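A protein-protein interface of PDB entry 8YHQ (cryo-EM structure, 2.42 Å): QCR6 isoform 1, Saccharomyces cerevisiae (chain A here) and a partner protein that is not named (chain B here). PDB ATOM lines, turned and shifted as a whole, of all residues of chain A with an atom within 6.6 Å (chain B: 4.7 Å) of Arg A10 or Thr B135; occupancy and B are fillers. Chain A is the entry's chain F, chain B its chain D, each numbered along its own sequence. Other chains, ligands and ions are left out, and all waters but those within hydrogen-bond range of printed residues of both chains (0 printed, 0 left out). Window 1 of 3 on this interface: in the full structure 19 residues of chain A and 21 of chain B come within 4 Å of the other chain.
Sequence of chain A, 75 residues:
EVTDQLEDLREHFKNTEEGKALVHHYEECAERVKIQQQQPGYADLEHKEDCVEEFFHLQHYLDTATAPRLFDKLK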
ATOM      1  N   ASP A   4     -11.334  -6.182  16.124  1.00  0.00           N
ATOM      2  CA  ASP A   4     -11.846  -7.537  16.038  1.00  0.00           C
ATOM      3  C   ASP A   4     -10.771  -8.456  15.464  1.00  0.00           C
ATOM      4  O   ASP A   4     -10.223  -8.212  14.389  1.00  0.00           O
ATOM      5  CB  ASP A   4     -13.098  -7.561  15.162  1.00  0.00           C
ATOM      6  CG  ASP A   4     -13.848  -8.860  15.250  1.00  0.00           C
ATOM      7  OD1 ASP A   4     -13.652  -9.580  16.242  1.00  0.00           O
ATOM      8  OD2 ASP A   4     -14.626  -9.167  14.321  1.00  0.00           O
ATOM      9  N   GLN A   5     -10.488  -9.539  16.186  1.00  0.00           N
ATOM     10  CA  GLN A   5      -9.320 -10.352  15.867  1.00  0.00           C
ATOM     11  C   GLN A   5      -9.463 -11.050  14.522  1.00  0.00           C
ATOM     12  O   GLN A   5      -8.469 -11.256  13.819  1.00  0.00           O
ATOM     13  CB  GLN A   5      -9.076 -11.382  16.966  1.00  0.00           C
ATOM     14  CG  GLN A   5      -8.704 -10.815  18.321  1.00  0.00           C
ATOM     15  CD  GLN A   5      -9.902 -10.430  19.152  1.00  0.00           C
ATOM     16  OE1 GLN A   5     -11.041 -10.582  18.723  1.00  0.00           O
ATOM     17  NE2 GLN A   5      -9.653  -9.939  20.352  1.00  0.00           N
ATOM     18  N   LEU A   6     -10.686 -11.423  14.146  1.00  0.00           N
ATOM     19  CA  LEU A   6     -10.903 -12.029  12.838  1.00  0.00           C
ATOM     20  C   LEU A   6     -10.601 -11.036  11.726  1.00  0.00           C
ATOM     21  O   LEU A   6      -9.991 -11.394  10.715  1.00  0.00           O
ATOM     22  CB  LEU A   6     -12.340 -12.540  12.745  1.00  0.00           C
ATOM     23  CG  LEU A   6     -12.858 -13.113  11.424  1.00  0.00           C
ATOM     24  CD1 LEU A   6     -11.936 -14.160  10.836  1.00  0.00           C
ATOM     25  CD2 LEU A   6     -14.235 -13.701  11.649  1.00  0.00           C
ATOM     26  N   GLU A   7     -11.006  -9.780  11.907  1.00  0.00           N
ATOM     27  CA  GLU A   7     -10.769  -8.747  10.904  1.00  0.00           C
ATOM     28  C   GLU A   7      -9.279  -8.547  10.648  1.00  0.00           C
ATOM     29  O   GLU A   7      -8.857  -8.313   9.511  1.00  0.00           O
ATOM     30  CB  GLU A   7     -11.427  -7.445  11.365  1.00  0.00           C
ATOM     31  CG  GLU A   7     -11.312  -6.233  10.433  1.00  0.00           C
ATOM     32  CD  GLU A   7     -11.423  -6.569   8.955  1.00  0.00           C
ATOM     33  OE1 GLU A   7     -12.554  -6.806   8.482  1.00  0.00           O
ATOM     34  OE2 GLU A   7     -10.386  -6.567   8.260  1.00  0.00           O
ATOM     35  N   ASP A   8      -8.462  -8.642  11.698  1.00  0.00           N
ATOM     36  CA  ASP A   8      -7.018  -8.530  11.521  1.00  0.00           C
ATOM     37  C   ASP A   8      -6.460  -9.699  10.719  1.00  0.00           C
ATOM     38  O   ASP A   8      -5.708  -9.496   9.760  1.00  0.00           O
ATOM     39  CB  ASP A   8      -6.328  -8.445  12.886  1.00  0.00           C
ATOM     40  CG  ASP A   8      -6.210  -7.017  13.413  1.00  0.00           C
ATOM     41  OD1 ASP A   8      -6.367  -6.049  12.641  1.00  0.00           O
ATOM     42  OD2 ASP A   8      -5.957  -6.864  14.626  1.00  0.00           O
ATOM     43  N   LEU A   9      -6.813 -10.931  11.092  1.00  0.00           N
ATOM     44  CA  LEU A   9      -6.340 -12.095  10.351  1.00  0.00           C
ATOM     45  C   LEU A   9      -6.963 -12.170   8.964  1.00  0.00           C
ATOM     46  O   LEU A   9      -6.270 -12.477   7.988  1.00  0.00           O
ATOM     47  CB  LEU A   9      -6.642 -13.370  11.132  1.00  0.00           C
ATOM     48  CG  LEU A   9      -5.550 -13.890  12.063  1.00  0.00           C
ATOM     49  CD1 LEU A   9      -5.128 -12.847  13.074  1.00  0.00           C
ATOM     50  CD2 LEU A   9      -6.050 -15.128  12.764  1.00  0.00           C
ATOM     51  N   ARG A  10      -8.260 -11.876   8.853  1.00  0.00           N
ATOM     52  CA  ARG A  10      -8.925 -11.816   7.557  1.00  0.00           C
ATOM     53  C   ARG A  10      -8.320 -10.759   6.640  1.00  0.00           C
ATOM     54  O   ARG A  10      -8.551 -10.813   5.427  1.00  0.00           O
ATOM     55  CB  ARG A  10     -10.420 -11.555   7.765  1.00  0.00           C
ATOM     56  CG  ARG A  10     -11.298 -11.858   6.582  1.00  0.00           C
ATOM     57  CD  ARG A  10     -12.744 -11.518   6.862  1.00  0.00           C
ATOM     58  NE  ARG A  10     -13.485 -12.652   7.407  1.00  0.00           N
ATOM     59  CZ  ARG A  10     -14.710 -12.584   7.921  1.00  0.00           C
ATOM     60  NH1 ARG A  10     -15.285 -13.681   8.377  1.00  0.00           N
ATOM     61  NH2 ARG A  10     -15.369 -11.437   7.991  1.00  0.00           N
ATOM     62  N   GLU A  11      -7.558  -9.809   7.186  1.00  0.00           N
ATOM     63  CA  GLU A  11      -6.819  -8.817   6.416  1.00  0.00           C
ATOM     64  C   GLU A  11      -5.337  -9.134   6.289  1.00  0.00           C
ATOM     65  O   GLU A  11      -4.684  -8.625   5.373  1.00  0.00           O
ATOM     66  CB  GLU A  11      -6.980  -7.436   7.059  1.00  0.00           C
ATOM     67  CG  GLU A  11      -6.484  -6.277   6.200  1.00  0.00           C
ATOM     68  CD  GLU A  11      -5.046  -5.857   6.487  1.00  0.00           C
ATOM     69  OE1 GLU A  11      -4.548  -6.073   7.613  1.00  0.00           O
ATOM     70  OE2 GLU A  11      -4.406  -5.301   5.569  1.00  0.00           O
ATOM     71  N   HIS A  12      -4.785  -9.950   7.189  1.00  0.00           N
ATOM     72  CA  HIS A  12      -3.382 -10.340   7.079  1.00  0.00           C
ATOM     73  C   HIS A  12      -3.174 -11.347   5.954  1.00  0.00           C
ATOM     74  O   HIS A  12      -2.374 -11.114   5.042  1.00  0.00           O
ATOM     75  CB  HIS A  12      -2.892 -10.906   8.412  1.00  0.00           C
ATOM     76  CG  HIS A  12      -1.618 -11.687   8.312  1.00  0.00           C
ATOM     77  ND1 HIS A  12      -1.464 -12.929   8.890  1.00  0.00           N
ATOM     78  CD2 HIS A  12      -0.435 -11.399   7.720  1.00  0.00           C
ATOM     79  CE1 HIS A  12      -0.244 -13.376   8.648  1.00  0.00           C
ATOM     80  NE2 HIS A  12       0.398 -12.467   7.938  1.00  0.00           N
ATOM     81  N   PHE A  13      -3.888 -12.476   5.997  1.00  0.00           N
ATOM     82  CA  PHE A  13      -3.774 -13.476   4.940  1.00  0.00           C
ATOM     83  C   PHE A  13      -4.293 -12.977   3.600  1.00  0.00           C
ATOM     84  O   PHE A  13      -4.036 -13.622   2.579  1.00  0.00           O
ATOM     85  CB  PHE A  13      -4.515 -14.752   5.338  1.00  0.00           C
ATOM     86  CG  PHE A  13      -3.986 -15.395   6.584  1.00  0.00           C
ATOM     87  CD1 PHE A  13      -2.809 -16.117   6.557  1.00  0.00           C
ATOM     88  CD2 PHE A  13      -4.663 -15.277   7.781  1.00  0.00           C
ATOM     89  CE1 PHE A  13      -2.320 -16.707   7.697  1.00  0.00           C
ATOM     90  CE2 PHE A  13      -4.178 -15.866   8.926  1.00  0.00           C
ATOM     91  CZ  PHE A  13      -3.005 -16.582   8.884  1.00  0.00           C
ATOM     92  N   LYS A  14      -4.996 -11.846   3.574  1.00  0.00           N
ATOM     93  CA  LYS A  14      -5.350 -11.152   2.345  1.00  0.00           C
ATOM     94  C   LYS A  14      -4.158 -10.444   1.696  1.00  0.00           C
ATOM     95  O   LYS A  14      -4.352  -9.755   0.689  1.00  0.00           O
ATOM     96  CB  LYS A  14      -6.467 -10.137   2.625  1.00  0.00           C
ATOM     97  CG  LYS A  14      -7.474  -9.981   1.501  1.00  0.00           C
ATOM     98  CD  LYS A  14      -8.310  -8.708   1.622  1.00  0.00           C
ATOM     99  CE  LYS A  14      -9.141  -8.647   2.892  1.00  0.00           C
ATOM    100  NZ  LYS A  14     -10.012  -9.824   3.081  1.00  0.00           N
ATOM    101  N   ASN A  15      -2.943 -10.591   2.245  1.00  0.00           N
ATOM    102  CA  ASN A  15      -1.721 -10.038   1.671  1.00  0.00           C
ATOM    103  C   ASN A  15      -0.635 -11.112   1.561  1.00  0.00           C
ATOM    104  O   ASN A  15       0.530 -10.879   1.893  1.00  0.00           O
ATOM    105  CB  ASN A  15      -1.259  -8.849   2.520  1.00  0.00           C
ATOM    106  CG  ASN A  15      -1.810  -7.534   2.021  1.00  0.00           C
ATOM    107  OD1 ASN A  15      -2.578  -6.868   2.715  1.00  0.00           O
ATOM    108  ND2 ASN A  15      -1.426  -7.150   0.813  1.00  0.00           N
ATOM    109  N   GLN A  59     -13.079 -15.697  -0.662  1.00  0.00           N
ATOM    110  CA  GLN A  59     -13.616 -15.871   0.681  1.00  0.00           C
ATOM    111  C   GLN A  59     -13.299 -17.255   1.236  1.00  0.00           C
ATOM    112  O   GLN A  59     -12.951 -17.397   2.412  1.00  0.00           O
ATOM    113  CB  GLN A  59     -15.120 -15.621   0.656  1.00  0.00           C
ATOM    114  CG  GLN A  59     -15.742 -15.356   2.002  1.00  0.00           C
ATOM    115  CD  GLN A  59     -15.524 -13.940   2.493  1.00  0.00           C
ATOM    116  OE1 GLN A  59     -14.837 -13.144   1.853  1.00  0.00           O
ATOM    117  NE2 GLN A  59     -16.119 -13.616   3.639  1.00  0.00           N
ATOM    118  N   LEU A  62      -9.443 -17.516   2.491  1.00  0.00           N
ATOM    119  CA  LEU A  62      -9.192 -16.802   3.738  1.00  0.00           C
ATOM    120  C   LEU A  62      -9.791 -17.526   4.936  1.00  0.00           C
ATOM    121  O   LEU A  62      -9.186 -17.564   6.011  1.00  0.00           O
ATOM    122  CB  LEU A  62      -9.768 -15.390   3.656  1.00  0.00           C
ATOM    123  CG  LEU A  62      -9.074 -14.321   2.815  1.00  0.00           C
ATOM    124  CD1 LEU A  62      -9.920 -13.079   2.816  1.00  0.00           C
ATOM    125  CD2 LEU A  62      -7.690 -13.995   3.324  1.00  0.00           C
ATOM    126  N   ASP A  63     -10.977 -18.112   4.771  1.00  0.00           N
ATOM    127  CA  ASP A  63     -11.672 -18.693   5.912  1.00  0.00           C
ATOM    128  C   ASP A  63     -11.023 -20.001   6.352  1.00  0.00           C
ATOM    129  O   ASP A  63     -10.757 -20.204   7.542  1.00  0.00           O
ATOM    130  CB  ASP A  63     -13.143 -18.911   5.576  1.00  0.00           C
ATOM    131  CG  ASP A  63     -13.909 -17.617   5.405  1.00  0.00           C
ATOM    132  OD1 ASP A  63     -13.513 -16.596   6.006  1.00  0.00           O
ATOM    133  OD2 ASP A  63     -14.920 -17.625   4.675  1.00  0.00           O
ATOM    134  N   THR A  66      -7.939 -19.192   7.977  1.00  0.00           N
ATOM    135  CA  THR A  66      -8.098 -18.432   9.208  1.00  0.00           C
ATOM    136  C   THR A  66      -8.922 -19.152  10.267  1.00  0.00           C
ATOM    137  O   THR A  66      -8.874 -18.758  11.437  1.00  0.00           O
ATOM    138  CB  THR A  66      -8.751 -17.078   8.891  1.00  0.00           C
ATOM    139  OG1 THR A  66      -8.075 -16.465   7.787  1.00  0.00           O
ATOM    140  CG2 THR A  66      -8.691 -16.153  10.070  1.00  0.00           C
ATOM    141  N   PHE B 131     -22.143 -18.513  13.572  1.00  0.00           N
ATOM    142  CA  PHE B 131     -21.032 -17.586  13.757  1.00  0.00           C
ATOM    143  C   PHE B 131     -20.640 -16.917  12.446  1.00  0.00           C
ATOM    144  O   PHE B 131     -20.447 -15.697  12.392  1.00  0.00           O
ATOM    145  CB  PHE B 131     -19.839 -18.333  14.357  1.00  0.00           C
ATOM    146  CG  PHE B 131     -18.661 -17.463  14.662  1.00  0.00           C
ATOM    147  CD1 PHE B 131     -18.538 -16.856  15.887  1.00  0.00           C
ATOM    148  CD2 PHE B 131     -17.668 -17.262  13.727  1.00  0.00           C
ATOM    149  CE1 PHE B 131     -17.464 -16.061  16.168  1.00  0.00           C
ATOM    150  CE2 PHE B 131     -16.596 -16.463  14.007  1.00  0.00           C
ATOM    151  CZ  PHE B 131     -16.493 -15.865  15.228  1.00  0.00           C
ATOM    152  N   SER B 132     -20.490 -17.706  11.381  1.00  0.00           N
ATOM    153  CA  SER B 132     -20.036 -17.163  10.107  1.00  0.00           C
ATOM    154  C   SER B 132     -21.057 -16.208   9.507  1.00  0.00           C
ATOM    155  O   SER B 132     -20.693 -15.277   8.782  1.00  0.00           O
ATOM    156  CB  SER B 132     -19.734 -18.302   9.142  1.00  0.00           C
ATOM    157  OG  SER B 132     -18.476 -18.877   9.409  1.00  0.00           O
ATOM    158  N   LEU B 133     -22.340 -16.429   9.787  1.00  0.00           N
ATOM    159  CA  LEU B 133     -23.380 -15.530   9.303  1.00  0.00           C
ATOM    160  C   LEU B 133     -23.238 -14.143   9.915  1.00  0.00           C
ATOM    161  O   LEU B 133     -23.182 -13.137   9.200  1.00  0.00           O
ATOM    162  CB  LEU B 133     -24.752 -16.122   9.617  1.00  0.00           C
ATOM    163  CG  LEU B 133     -25.998 -15.490   9.004  1.00  0.00           C
ATOM    164  CD1 LEU B 133     -26.095 -15.774   7.522  1.00  0.00           C
ATOM    165  CD2 LEU B 133     -27.225 -15.993   9.725  1.00  0.00           C
ATOM    166  N   LEU B 134     -23.175 -14.075  11.244  1.00  0.00           N
ATOM    167  CA  LEU B 134     -23.152 -12.798  11.945  1.00  0.00           C
ATOM    168  C   LEU B 134     -21.894 -11.993  11.644  1.00  0.00           C
ATOM    169  O   LEU B 134     -21.927 -10.760  11.703  1.00  0.00           O
ATOM    170  CB  LEU B 134     -23.272 -13.043  13.440  1.00  0.00           C
ATOM    171  CG  LEU B 134     -24.568 -13.689  13.923  1.00  0.00           C
ATOM    172  CD1 LEU B 134     -24.405 -14.260  15.306  1.00  0.00           C
ATOM    173  CD2 LEU B 134     -25.710 -12.709  13.915  1.00  0.00           C
ATOM    174  N   THR B 135     -20.786 -12.664  11.329  1.00  0.00           N
ATOM    175  CA  THR B 135     -19.504 -12.021  11.064  1.00  0.00           C
ATOM    176  C   THR B 135     -19.164 -11.978   9.576  1.00  0.00           C
ATOM    177  O   THR B 135     -18.006 -11.748   9.220  1.00  0.00           O
ATOM    178  CB  THR B 135     -18.396 -12.737  11.834  1.00  0.00           C
ATOM    179  OG1 THR B 135     -18.529 -14.150  11.668  1.00  0.00           O
ATOM    180  CG2 THR B 135     -18.462 -12.412  13.302  1.00  0.00           C
ATOM    181  N   GLY B 136     -20.152 -12.165   8.705  1.00  0.00           N
ATOM    182  CA  GLY B 136     -19.913 -12.332   7.284  1.00  0.00           C
ATOM    183  C   GLY B 136     -20.427 -11.232   6.381  1.00  0.00           C
ATOM    184  O   GLY B 136     -20.251 -11.311   5.163  1.00  0.00           O
ATOM    185  N   TYR B 137     -21.055 -10.211   6.945  1.00  0.00           N
ATOM    186  CA  TYR B 137     -21.580  -9.113   6.144  1.00  0.00           C
ATOM    187  C   TYR B 137     -20.425  -8.319   5.541  1.00  0.00           C
ATOM    188  O   TYR B 137     -19.617  -7.769   6.297  1.00  0.00           O
ATOM    189  CB  TYR B 137     -22.446  -8.201   6.998  1.00  0.00           C
ATOM    190  CG  TYR B 137     -23.802  -8.766   7.336  1.00  0.00           C
ATOM    191  CD1 TYR B 137     -24.881  -8.575   6.496  1.00  0.00           C
ATOM    192  CD2 TYR B 137     -24.008  -9.479   8.501  1.00  0.00           C
ATOM    193  CE1 TYR B 137     -26.116  -9.083   6.805  1.00  0.00           C
ATOM    194  CE2 TYR B 137     -25.237  -9.988   8.813  1.00  0.00           C
ATOM    195  CZ  TYR B 137     -26.287  -9.789   7.968  1.00  0.00           C
ATOM    196  OH  TYR B 137     -27.512 -10.306   8.297  1.00  0.00           O
ATOM    197  N   THR B 183     -16.488  -7.598  18.040  1.00  0.00           N
ATOM    198  CA  THR B 183     -17.545  -8.211  17.244  1.00  0.00           C
ATOM    199  C   THR B 183     -17.497  -9.734  17.328  1.00  0.00           C
ATOM    200  O   THR B 183     -18.525 -10.387  17.536  1.00  0.00           O
ATOM    201  CB  THR B 183     -17.424  -7.743  15.795  1.00  0.00           C
ATOM    202  OG1 THR B 183     -17.551  -6.320  15.741  1.00  0.00           O
ATOM    203  CG2 THR B 183     -18.487  -8.370  14.926  1.00  0.00           C
ATOM    204  N   SER B 184     -16.309 -10.317  17.160  1.00  0.00           N
ATOM    205  CA  SER B 184     -16.185 -11.770  17.182  1.00  0.00           C
ATOM    206  C   SER B 184     -16.450 -12.330  18.570  1.00  0.00           C
ATOM    207  O   SER B 184     -17.013 -13.421  18.710  1.00  0.00           O
ATOM    208  CB  SER B 184     -14.798 -12.184  16.709  1.00  0.00           C
ATOM    209  OG  SER B 184     -14.583 -11.792  15.367  1.00  0.00           O
ATOM    210  N   ALA B 187     -20.182 -12.562  19.130  1.00  0.00           N
ATOM    211  CA  ALA B 187     -20.745 -13.588  18.259  1.00  0.00           C
ATOM    212  C   ALA B 187     -20.483 -14.985  18.808  1.00  0.00           C
ATOM    213  O   ALA B 187     -21.354 -15.860  18.751  1.00  0.00           O
ATOM    214  CB  ALA B 187     -20.169 -13.449  16.852  1.00  0.00           C
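NZ of Lys A14 lies within hydrogen-bond range of O of Arg A10 (2.9 Å).
O of Phe B131 sits at hydrogen-bond distance from OG1 of Thr B135, at 2.6 Å.
Of the 10 printed residues of chain B, 3 touch a printed residue of chain A.
Printed residues of chain A that touch a printed residue of chain B: Asp A4, Leu A6 and Arg A10.
Hydrophobic or aromatic side chains of chain A within 4 Å of the printed part of chain B: Leu A6.
Among the printed residues, no Asp or Glu carboxylate lies within 4 Å of a Lys or Arg side-chain nitrogen of the other chain.
Of chain B, only Thr B135 (2.9 Å) comes within 4 Å of Arg A10.
Thr B135 touches one residue of chain A.
Printed residues of chain A within 4 Å of Thr B183: Asp A4 (3.5 Å).
Printed residues of chain A within 4 Å of Ser B184: Asp A4 (2.6 Å) and Leu A6 (3.5 Å).
The nearest printed residue of chain A that does not touch Ser B184 is Gln A5 (4.6 Å).
Asp A4 touches Thr B183.
Leu A6 touches Ser B184 (CB to OG, 3.5 Å).
OD1 of Asp A4 lies within hydrogen-bond range of OG of Ser B184 (2.6 Å).
O of Thr B135 is in hydrogen-bond range of NH2 of Arg A10, at 2.9 Å.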
